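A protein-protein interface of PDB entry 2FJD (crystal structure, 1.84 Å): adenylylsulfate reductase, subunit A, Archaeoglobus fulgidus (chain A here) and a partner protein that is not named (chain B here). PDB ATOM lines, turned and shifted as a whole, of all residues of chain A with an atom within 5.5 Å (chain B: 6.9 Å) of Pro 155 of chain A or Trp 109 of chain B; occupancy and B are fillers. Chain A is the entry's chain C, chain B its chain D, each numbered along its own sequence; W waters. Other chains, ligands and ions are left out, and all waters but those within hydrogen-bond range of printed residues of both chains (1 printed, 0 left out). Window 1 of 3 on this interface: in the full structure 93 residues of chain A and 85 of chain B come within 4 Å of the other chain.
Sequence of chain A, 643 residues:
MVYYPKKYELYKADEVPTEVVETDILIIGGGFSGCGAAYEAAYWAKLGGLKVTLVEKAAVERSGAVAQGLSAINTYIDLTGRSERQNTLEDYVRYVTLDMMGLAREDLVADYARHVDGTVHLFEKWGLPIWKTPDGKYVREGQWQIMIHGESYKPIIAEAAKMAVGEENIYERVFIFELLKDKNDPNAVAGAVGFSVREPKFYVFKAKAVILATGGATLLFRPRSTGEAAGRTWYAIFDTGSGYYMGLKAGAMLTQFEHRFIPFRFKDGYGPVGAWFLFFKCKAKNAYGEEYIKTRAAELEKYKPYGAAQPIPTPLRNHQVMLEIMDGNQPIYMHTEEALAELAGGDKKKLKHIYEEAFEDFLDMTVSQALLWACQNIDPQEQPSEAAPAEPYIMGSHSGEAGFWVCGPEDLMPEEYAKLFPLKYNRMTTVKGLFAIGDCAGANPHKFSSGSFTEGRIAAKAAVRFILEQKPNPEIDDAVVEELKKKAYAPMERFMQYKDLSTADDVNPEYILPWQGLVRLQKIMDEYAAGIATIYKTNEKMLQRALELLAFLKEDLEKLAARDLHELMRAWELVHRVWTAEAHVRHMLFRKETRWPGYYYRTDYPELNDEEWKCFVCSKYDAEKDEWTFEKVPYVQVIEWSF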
ATOM      1  N   GLU A  61      24.236 -20.035 -19.146  1.00  0.00           N
ATOM      2  CA  GLU A  61      24.675 -19.690 -17.793  1.00  0.00           C
ATOM      3  C   GLU A  61      23.593 -19.013 -16.945  1.00  0.00           C
ATOM      4  O   GLU A  61      23.492 -19.271 -15.744  1.00  0.00           O
ATOM      5  CB  GLU A  61      25.907 -18.777 -17.841  1.00  0.00           C
ATOM      6  CG  GLU A  61      26.550 -18.559 -16.475  1.00  0.00           C
ATOM      7  CD  GLU A  61      27.792 -17.683 -16.530  1.00  0.00           C
ATOM      8  OE1 GLU A  61      28.419 -17.603 -17.607  1.00  0.00           O
ATOM      9  OE2 GLU A  61      28.145 -17.089 -15.487  1.00  0.00           O
ATOM     10  N   ARG A  62      22.787 -18.155 -17.566  1.00  0.00           N
ATOM     11  CA  ARG A  62      21.734 -17.434 -16.841  1.00  0.00           C
ATOM     12  C   ARG A  62      20.374 -17.396 -17.537  1.00  0.00           C
ATOM     13  O   ARG A  62      19.469 -16.707 -17.073  1.00  0.00           O
ATOM     14  CB  ARG A  62      22.177 -15.986 -16.598  1.00  0.00           C
ATOM     15  CG  ARG A  62      23.283 -15.816 -15.572  1.00  0.00           C
ATOM     16  CD  ARG A  62      22.741 -15.922 -14.158  1.00  0.00           C
ATOM     17  NE  ARG A  62      23.824 -15.860 -13.184  1.00  0.00           N
ATOM     18  CZ  ARG A  62      23.653 -15.816 -11.868  1.00  0.00           C
ATOM     19  NH1 ARG A  62      22.430 -15.822 -11.346  1.00  0.00           N
ATOM     20  NH2 ARG A  62      24.714 -15.773 -11.070  1.00  0.00           N
ATOM     21  N   VAL A  66      15.246 -19.000 -14.078  1.00  0.00           N
ATOM     22  CA  VAL A  66      16.150 -19.017 -12.930  1.00  0.00           C
ATOM     23  C   VAL A  66      17.341 -18.064 -13.067  1.00  0.00           C
ATOM     24  O   VAL A  66      18.352 -18.205 -12.375  1.00  0.00           O
ATOM     25  CB  VAL A  66      16.648 -20.464 -12.664  1.00  0.00           C
ATOM     26  CG1 VAL A  66      17.411 -20.538 -11.338  1.00  0.00           C
ATOM     27  CG2 VAL A  66      15.455 -21.414 -12.632  1.00  0.00           C
ATOM     28  N   GLU A 151      21.414 -18.344  -5.424  1.00  0.00           N
ATOM     29  CA  GLU A 151      21.743 -17.255  -6.330  1.00  0.00           C
ATOM     30  C   GLU A 151      22.357 -17.804  -7.620  1.00  0.00           C
ATOM     31  O   GLU A 151      22.066 -17.311  -8.710  1.00  0.00           O
ATOM     32  CB  GLU A 151      22.723 -16.281  -5.663  1.00  0.00           C
ATOM     33  CG  GLU A 151      23.052 -15.056  -6.513  1.00  0.00           C
ATOM     34  CD  GLU A 151      24.114 -15.314  -7.572  1.00  0.00           C
ATOM     35  OE1 GLU A 151      24.077 -14.644  -8.627  1.00  0.00           O
ATOM     36  OE2 GLU A 151      24.995 -16.172  -7.347  1.00  0.00           O
ATOM     37  N   SER A 152      23.200 -18.829  -7.490  1.00  0.00           N
ATOM     38  CA  SER A 152      23.861 -19.432  -8.651  1.00  0.00           C
ATOM     39  C   SER A 152      23.218 -20.736  -9.102  1.00  0.00           C
ATOM     40  O   SER A 152      23.860 -21.555  -9.756  1.00  0.00           O
ATOM     41  CB  SER A 152      25.345 -19.687  -8.350  1.00  0.00           C
ATOM     42  OG  SER A 152      26.067 -18.472  -8.284  1.00  0.00           O
ATOM     43  N   TYR A 153      21.947 -20.913  -8.764  1.00  0.00           N
ATOM     44  CA  TYR A 153      21.211 -22.118  -9.119  1.00  0.00           C
ATOM     45  C   TYR A 153      21.328 -22.457 -10.607  1.00  0.00           C
ATOM     46  O   TYR A 153      21.642 -23.590 -10.969  1.00  0.00           O
ATOM     47  CB  TYR A 153      19.744 -21.928  -8.729  1.00  0.00           C
ATOM     48  CG  TYR A 153      18.890 -23.180  -8.670  1.00  0.00           C
ATOM     49  CD1 TYR A 153      19.449 -24.461  -8.737  1.00  0.00           C
ATOM     50  CD2 TYR A 153      17.510 -23.073  -8.511  1.00  0.00           C
ATOM     51  CE1 TYR A 153      18.641 -25.605  -8.645  1.00  0.00           C
ATOM     52  CE2 TYR A 153      16.700 -24.196  -8.416  1.00  0.00           C
ATOM     53  CZ  TYR A 153      17.263 -25.457  -8.484  1.00  0.00           C
ATOM     54  OH  TYR A 153      16.428 -26.551  -8.396  1.00  0.00           O
ATOM     55  N   LYS A 154      21.080 -21.481 -11.474  1.00  0.00           N
ATOM     56  CA  LYS A 154      21.161 -21.743 -12.909  1.00  0.00           C
ATOM     57  C   LYS A 154      22.607 -21.973 -13.365  1.00  0.00           C
ATOM     58  O   LYS A 154      22.875 -22.898 -14.124  1.00  0.00           O
ATOM     59  CB  LYS A 154      20.519 -20.606 -13.719  1.00  0.00           C
ATOM     60  CG  LYS A 154      20.469 -20.885 -15.227  1.00  0.00           C
ATOM     61  CD  LYS A 154      19.607 -22.108 -15.565  1.00  0.00           C
ATOM     62  CE  LYS A 154      19.907 -22.656 -16.967  1.00  0.00           C
ATOM     63  NZ  LYS A 154      19.710 -21.661 -18.059  1.00  0.00           N
ATOM     64  N   PRO A 155      23.556 -21.118 -12.947  1.00  0.00           N
ATOM     65  CA  PRO A 155      24.945 -21.331 -13.375  1.00  0.00           C
ATOM     66  C   PRO A 155      25.456 -22.738 -13.047  1.00  0.00           C
ATOM     67  O   PRO A 155      26.197 -23.343 -13.827  1.00  0.00           O
ATOM     68  CB  PRO A 155      25.706 -20.251 -12.614  1.00  0.00           C
ATOM     69  CG  PRO A 155      24.727 -19.134 -12.576  1.00  0.00           C
ATOM     70  CD  PRO A 155      23.419 -19.829 -12.244  1.00  0.00           C
ATOM     71  N   ILE A 156      25.068 -23.249 -11.884  1.00  0.00           N
ATOM     72  CA  ILE A 156      25.481 -24.581 -11.465  1.00  0.00           C
ATOM     73  C   ILE A 156      24.883 -25.633 -12.398  1.00  0.00           C
ATOM     74  O   ILE A 156      25.581 -26.525 -12.875  1.00  0.00           O
ATOM     75  CB  ILE A 156      25.044 -24.853 -10.004  1.00  0.00           C
ATOM     76  CG1 ILE A 156      25.810 -23.916  -9.066  1.00  0.00           C
ATOM     77  CG2 ILE A 156      25.307 -26.312  -9.629  1.00  0.00           C
ATOM     78  CD1 ILE A 156      25.407 -24.020  -7.613  1.00  0.00           C
ATOM     79  N   ILE A 157      23.589 -25.518 -12.667  1.00  0.00           N
ATOM     80  CA  ILE A 157      22.916 -26.459 -13.549  1.00  0.00           C
ATOM     81  C   ILE A 157      23.449 -26.340 -14.978  1.00  0.00           C
ATOM     82  O   ILE A 157      23.556 -27.337 -15.694  1.00  0.00           O
ATOM     83  CB  ILE A 157      21.375 -26.243 -13.502  1.00  0.00           C
ATOM     84  CG1 ILE A 157      20.774 -27.152 -12.427  1.00  0.00           C
ATOM     85  CG2 ILE A 157      20.739 -26.536 -14.854  1.00  0.00           C
ATOM     86  CD1 ILE A 157      21.403 -26.993 -11.058  1.00  0.00           C
ATOM     87  N   ALA A 158      23.796 -25.126 -15.387  1.00  0.00           N
ATOM     88  CA  ALA A 158      24.334 -24.912 -16.725  1.00  0.00           C
ATOM     89  C   ALA A 158      25.684 -25.620 -16.838  1.00  0.00           C
ATOM     90  O   ALA A 158      25.998 -26.230 -17.863  1.00  0.00           O
ATOM     91  CB  ALA A 158      24.497 -23.420 -16.996  1.00  0.00           C
ATOM     92  N   GLU A 159      26.481 -25.534 -15.778  1.00  0.00           N
ATOM     93  CA  GLU A 159      27.794 -26.167 -15.762  1.00  0.00           C
ATOM     94  C   GLU A 159      27.645 -27.677 -15.915  1.00  0.00           C
ATOM     95  O   GLU A 159      28.379 -28.305 -16.677  1.00  0.00           O
ATOM     96  CB  GLU A 159      28.532 -25.849 -14.457  1.00  0.00           C
ATOM     97  CG  GLU A 159      29.897 -26.540 -14.337  1.00  0.00           C
ATOM     98  CD  GLU A 159      30.639 -26.183 -13.059  1.00  0.00           C
ATOM     99  OE1 GLU A 159      31.158 -27.108 -12.393  1.00  0.00           O
ATOM    100  OE2 GLU A 159      30.712 -24.982 -12.720  1.00  0.00           O
ATOM    101  N   ALA A 160      26.689 -28.255 -15.192  1.00  0.00           N
ATOM    102  CA  ALA A 160      26.462 -29.692 -15.260  1.00  0.00           C
ATOM    103  C   ALA A 160      26.089 -30.104 -16.680  1.00  0.00           C
ATOM    104  O   ALA A 160      26.622 -31.080 -17.214  1.00  0.00           O
ATOM    105  CB  ALA A 160      25.353 -30.096 -14.280  1.00  0.00           C
ATOM    106  N   ILE B  24      25.906 -12.268 -21.160  1.00  0.00           N
ATOM    107  CA  ILE B  24      25.021 -12.817 -20.135  1.00  0.00           C
ATOM    108  C   ILE B  24      23.517 -12.503 -20.169  1.00  0.00           C
ATOM    109  O   ILE B  24      22.714 -13.346 -19.773  1.00  0.00           O
ATOM    110  CB  ILE B  24      25.564 -12.445 -18.724  1.00  0.00           C
ATOM    111  CG1 ILE B  24      25.092 -13.460 -17.679  1.00  0.00           C
ATOM    112  CG2 ILE B  24      25.107 -11.046 -18.342  1.00  0.00           C
ATOM    113  CD1 ILE B  24      25.741 -14.830 -17.813  1.00  0.00           C
ATOM    114  N   ARG B  81      29.510 -10.381  -6.085  1.00  0.00           N
ATOM    115  CA  ARG B  81      29.515 -11.829  -6.213  1.00  0.00           C
ATOM    116  C   ARG B  81      30.913 -12.430  -6.262  1.00  0.00           C
ATOM    117  O   ARG B  81      31.736 -12.048  -7.092  1.00  0.00           O
ATOM    118  CB  ARG B  81      28.719 -12.216  -7.465  1.00  0.00           C
ATOM    119  CG  ARG B  81      28.536 -13.702  -7.693  1.00  0.00           C
ATOM    120  CD  ARG B  81      27.370 -13.937  -8.643  1.00  0.00           C
ATOM    121  NE  ARG B  81      27.232 -15.337  -9.026  1.00  0.00           N
ATOM    122  CZ  ARG B  81      28.025 -15.957  -9.893  1.00  0.00           C
ATOM    123  NH1 ARG B  81      29.019 -15.299 -10.479  1.00  0.00           N
ATOM    124  NH2 ARG B  81      27.830 -17.240 -10.170  1.00  0.00           N
ATOM    125  N   GLY B  82      31.166 -13.374  -5.360  1.00  0.00           N
ATOM    126  CA  GLY B  82      32.456 -14.032  -5.304  1.00  0.00           C
ATOM    127  C   GLY B  82      32.376 -15.432  -5.878  1.00  0.00           C
ATOM    128  O   GLY B  82      31.619 -15.680  -6.817  1.00  0.00           O
ATOM    129  N   THR B  83      33.150 -16.352  -5.311  1.00  0.00           N
ATOM    130  CA  THR B  83      33.159 -17.729  -5.787  1.00  0.00           C
ATOM    131  C   THR B  83      32.321 -18.662  -4.916  1.00  0.00           C
ATOM    132  O   THR B  83      31.701 -19.600  -5.420  1.00  0.00           O
ATOM    133  CB  THR B  83      34.595 -18.276  -5.853  1.00  0.00           C
ATOM    134  OG1 THR B  83      35.219 -18.115  -4.574  1.00  0.00           O
ATOM    135  CG2 THR B  83      35.402 -17.527  -6.899  1.00  0.00           C
ATOM    136  N   SER B  84      32.295 -18.408  -3.610  1.00  0.00           N
ATOM    137  CA  SER B  84      31.528 -19.254  -2.700  1.00  0.00           C
ATOM    138  C   SER B  84      30.353 -18.515  -2.072  1.00  0.00           C
ATOM    139  O   SER B  84      29.440 -19.135  -1.524  1.00  0.00           O
ATOM    140  CB  SER B  84      32.439 -19.803  -1.599  1.00  0.00           C
ATOM    141  OG  SER B  84      32.961 -18.756  -0.801  1.00  0.00           O
ATOM    142  N   ASP B  85      30.378 -17.189  -2.143  1.00  0.00           N
ATOM    143  CA  ASP B  85      29.299 -16.389  -1.583  1.00  0.00           C
ATOM    144  C   ASP B  85      29.072 -15.092  -2.348  1.00  0.00           C
ATOM    145  O   ASP B  85      29.820 -14.748  -3.266  1.00  0.00           O
ATOM    146  CB  ASP B  85      29.575 -16.072  -0.109  1.00  0.00           C
ATOM    147  CG  ASP B  85      30.964 -15.512   0.120  1.00  0.00           C
ATOM    148  OD1 ASP B  85      31.375 -14.603  -0.635  1.00  0.00           O
ATOM    149  OD2 ASP B  85      31.641 -15.975   1.063  1.00  0.00           O
ATOM    150  N   ILE B 104      26.722 -19.184  -2.143  1.00  0.00           N
ATOM    151  CA  ILE B 104      26.189 -19.432  -3.483  1.00  0.00           C
ATOM    152  C   ILE B 104      26.652 -20.772  -4.059  1.00  0.00           C
ATOM    153  O   ILE B 104      26.031 -21.306  -4.979  1.00  0.00           O
ATOM    154  CB  ILE B 104      26.554 -18.301  -4.483  1.00  0.00           C
ATOM    155  CG1 ILE B 104      28.066 -18.245  -4.703  1.00  0.00           C
ATOM    156  CG2 ILE B 104      26.027 -16.972  -3.966  1.00  0.00           C
ATOM    157  CD1 ILE B 104      28.485 -17.221  -5.747  1.00  0.00           C
ATOM    158  N   ARG B 105      27.742 -21.317  -3.527  1.00  0.00           N
ATOM    159  CA  ARG B 105      28.231 -22.612  -4.000  1.00  0.00           C
ATOM    160  C   ARG B 105      29.175 -23.249  -2.983  1.00  0.00           C
ATOM    161  O   ARG B 105      29.992 -22.562  -2.370  1.00  0.00           O
ATOM    162  CB  ARG B 105      28.933 -22.475  -5.357  1.00  0.00           C
ATOM    163  CG  ARG B 105      29.266 -23.825  -5.981  1.00  0.00           C
ATOM    164  CD  ARG B 105      29.682 -23.719  -7.436  1.00  0.00           C
ATOM    165  NE  ARG B 105      30.017 -25.033  -7.981  1.00  0.00           N
ATOM    166  CZ  ARG B 105      30.125 -25.303  -9.278  1.00  0.00           C
ATOM    167  NH1 ARG B 105      29.920 -24.351 -10.174  1.00  0.00           N
ATOM    168  NH2 ARG B 105      30.447 -26.525  -9.679  1.00  0.00           N
ATOM    169  N   THR B 107      31.156 -25.977  -3.809  1.00  0.00           N
ATOM    170  CA  THR B 107      32.240 -26.651  -4.522  1.00  0.00           C
ATOM    171  C   THR B 107      32.924 -25.669  -5.464  1.00  0.00           C
ATOM    172  O   THR B 107      32.360 -24.626  -5.798  1.00  0.00           O
ATOM    173  CB  THR B 107      31.718 -27.833  -5.365  1.00  0.00           C
ATOM    174  OG1 THR B 107      30.785 -27.346  -6.337  1.00  0.00           O
ATOM    175  CG2 THR B 107      31.036 -28.867  -4.480  1.00  0.00           C
ATOM    176  N   PRO B 108      34.149 -25.991  -5.910  1.00  0.00           N
ATOM    177  CA  PRO B 108      34.875 -25.100  -6.822  1.00  0.00           C
ATOM    178  C   PRO B 108      34.163 -24.992  -8.163  1.00  0.00           C
ATOM    179  O   PRO B 108      33.573 -25.961  -8.639  1.00  0.00           O
ATOM    180  CB  PRO B 108      36.240 -25.775  -6.958  1.00  0.00           C
ATOM    181  CG  PRO B 108      36.381 -26.537  -5.667  1.00  0.00           C
ATOM    182  CD  PRO B 108      34.999 -27.121  -5.497  1.00  0.00           C
ATOM    183  N   TRP B 109      34.220 -23.819  -8.781  1.00  0.00           N
ATOM    184  CA  TRP B 109      33.571 -23.642 -10.068  1.00  0.00           C
ATOM    185  C   TRP B 109      34.231 -24.499 -11.136  1.00  0.00           C
ATOM    186  O   TRP B 109      35.458 -24.613 -11.183  1.00  0.00           O
ATOM    187  CB  TRP B 109      33.579 -22.166 -10.473  1.00  0.00           C
ATOM    188  CG  TRP B 109      32.552 -21.396  -9.722  1.00  0.00           C
ATOM    189  CD1 TRP B 109      32.683 -20.845  -8.481  1.00  0.00           C
ATOM    190  CD2 TRP B 109      31.185 -21.210 -10.102  1.00  0.00           C
ATOM    191  NE1 TRP B 109      31.480 -20.333  -8.060  1.00  0.00           N
ATOM    192  CE2 TRP B 109      30.542 -20.544  -9.035  1.00  0.00           C
ATOM    193  CE3 TRP B 109      30.438 -21.546 -11.239  1.00  0.00           C
ATOM    194  CZ2 TRP B 109      29.185 -20.209  -9.072  1.00  0.00           C
ATOM    195  CZ3 TRP B 109      29.087 -21.214 -11.276  1.00  0.00           C
ATOM    196  CH2 TRP B 109      28.476 -20.551 -10.195  1.00  0.00           C
ATOM    197  N   GLY B 110      33.400 -25.121 -11.967  1.00  0.00           N
ATOM    198  CA  GLY B 110      33.887 -25.975 -13.039  1.00  0.00           C
ATOM    199  C   GLY B 110      34.367 -27.333 -12.569  1.00  0.00           C
ATOM    200  O   GLY B 110      35.051 -28.039 -13.307  1.00  0.00           O
ATOM    201  N   SER B 111      33.992 -27.718 -11.354  1.00  0.00           N
ATOM    202  CA  SER B 111      34.433 -28.991 -10.795  1.00  0.00           C
ATOM    203  C   SER B 111      33.450 -30.145 -10.938  1.00  0.00           C
ATOM    204  O   SER B 111      33.747 -31.265 -10.526  1.00  0.00           O
ATOM    205  CB  SER B 111      34.767 -28.815  -9.313  1.00  0.00           C
ATOM    206  OG  SER B 111      33.609 -28.451  -8.582  1.00  0.00           O
ATOM    207  N   ILE B 112      32.282 -29.885 -11.513  1.00  0.00           N
ATOM    208  CA  ILE B 112      31.289 -30.942 -11.665  1.00  0.00           C
ATOM    209  C   ILE B 112      31.708 -32.067 -12.609  1.00  0.00           C
ATOM    210  O   ILE B 112      32.168 -31.826 -13.726  1.00  0.00           O
ATOM    211  CB  ILE B 112      29.932 -30.379 -12.169  1.00  0.00           C
ATOM    212  CG1 ILE B 112      29.315 -29.464 -11.110  1.00  0.00           C
ATOM    213  CG2 ILE B 112      28.981 -31.529 -12.496  1.00  0.00           C
ATOM    214  CD1 ILE B 112      28.064 -28.736 -11.577  1.00  0.00           C
HETATM  215  O   HOH W   1      23.545 -20.948  -5.539  1.00  0.00           O
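The side-chain carboxylate of Glu 151 of chain A lies within salt-bridge range of the guanidinium group of Arg 62 of chain A (2.8 Å).
The side-chain carboxylate (OE2) of Glu 151 of chain A sits at hydrogen-bond distance from the side-chain hydroxyl (OG) of Ser 152 of chain A (2.7 Å).
O of Ser 84 of chain B is in hydrogen-bond range of N of Ile 104 of chain B, 2.8 Å away.
The backbone carbonyl oxygen of Ser 84 of chain B is in hydrogen-bond range of the backbone NH of Arg 105 of chain B (3.4 Å).
The guanidinium group (NH2) of Arg 105 of chain B sits at hydrogen-bond distance from the backbone carbonyl oxygen (O) of Pro 108 of chain B (3.3 Å).
The backbone carbonyl oxygen (O) of Pro 108 of chain B is in hydrogen-bond range of the side-chain hydroxyl (OG) of Ser 111 of chain B (2.5 Å).
Water W1 lies within hydrogen-bond range of O of Ile 104 of chain B (2.6 Å), N of Ser 152 of chain A (2.9 Å) and N of Glu 151 of chain A (3.4 Å).
Of the printed residues of chain B, Pro 155 of chain A touches Trp 109 (3.7 Å).
Of the printed residues of chain A, Ser 111 of chain B touches Glu 159.
Of the printed residues of chain A, Arg 105 of chain B touches Glu 159 (2.7 Å).
Lys 154 of chain A touches none of the printed residues of chain B.
Among the printed residues, merely in contact across the chains: Arg 62 of chain A with Ile 24 of chain B (3.5 Å), Ile 156 of chain A with Ile 112 of chain B (3.6 Å), Glu 151 of chain A with Ile 104 of chain B (3.6 Å), Ser 152 of chain A with Trp 109 of chain B (3.7 Å), Pro 155 of chain A with Trp 109 of chain B (3.7 Å), Ser 152 of chain A with Ile 104 of chain B (3.7 Å), Glu 61 of chain A with Ile 24 of chain B (3.7 Å), Glu 159 of chain A with Trp 109 of chain B (3.8 Å), Ile 156 of chain A with Ile 104 of chain B (3.8 Å) and Ala 160 of chain A with Ile 112 of chain B (3.9 Å).
The side-chain carboxylate of Glu 151 of chain A lies within salt-bridge range of the guanidinium group of Arg 81 of chain B, at 2.9 Å.
NH2 of Arg 81 of chain B is in hydrogen-bond range of OG of Ser 152 of chain A (2.9 Å).
The guanidinium group of Arg 105 of chain B lies within salt-bridge range of the side-chain carboxylate of Glu 159 of chain A, at 2.7 Å.
OE2 of Glu 159 of chain A is in hydrogen-bond range of N of Gly 110 of chain B (2.8 Å).
OE1 of Glu 159 of chain A sits at hydrogen-bond distance from N of Ser 111 of chain B (3.1 Å).
The side-chain carboxylate of Glu 159 of chain A sits at hydrogen-bond distance from the backbone NH of Ile 112 of chain B (3.1 Å).
NH2 of Arg 62 of chain A lies close to NE of Arg 81 of chain B (3.3 Å).
Of the 14 printed residues of chain B, 8 touch a printed residue of chain A.
Printed residues of chain B that touch a printed residue of chain A: Ile 24, Arg 81, Ile 104, Arg 105, Trp 109, Gly 110, Ser 111 and Ile 112.
Hydrophobic or aromatic side chains of chain B within 4 Å of the printed part of chain A: Ile 24, Ile 104, Trp 109 and Ile 112.
Along chain B the printed residues that touch a printed residue of chain A span positions 24 to 112.
Among the printed residues, Asp or Glu carboxylates within 4 Å of a Lys or Arg side-chain nitrogen of the other chain: Glu 151 of chain A with Arg 81 of chain B and Glu 159 of chain A with Arg 105 of chain B.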
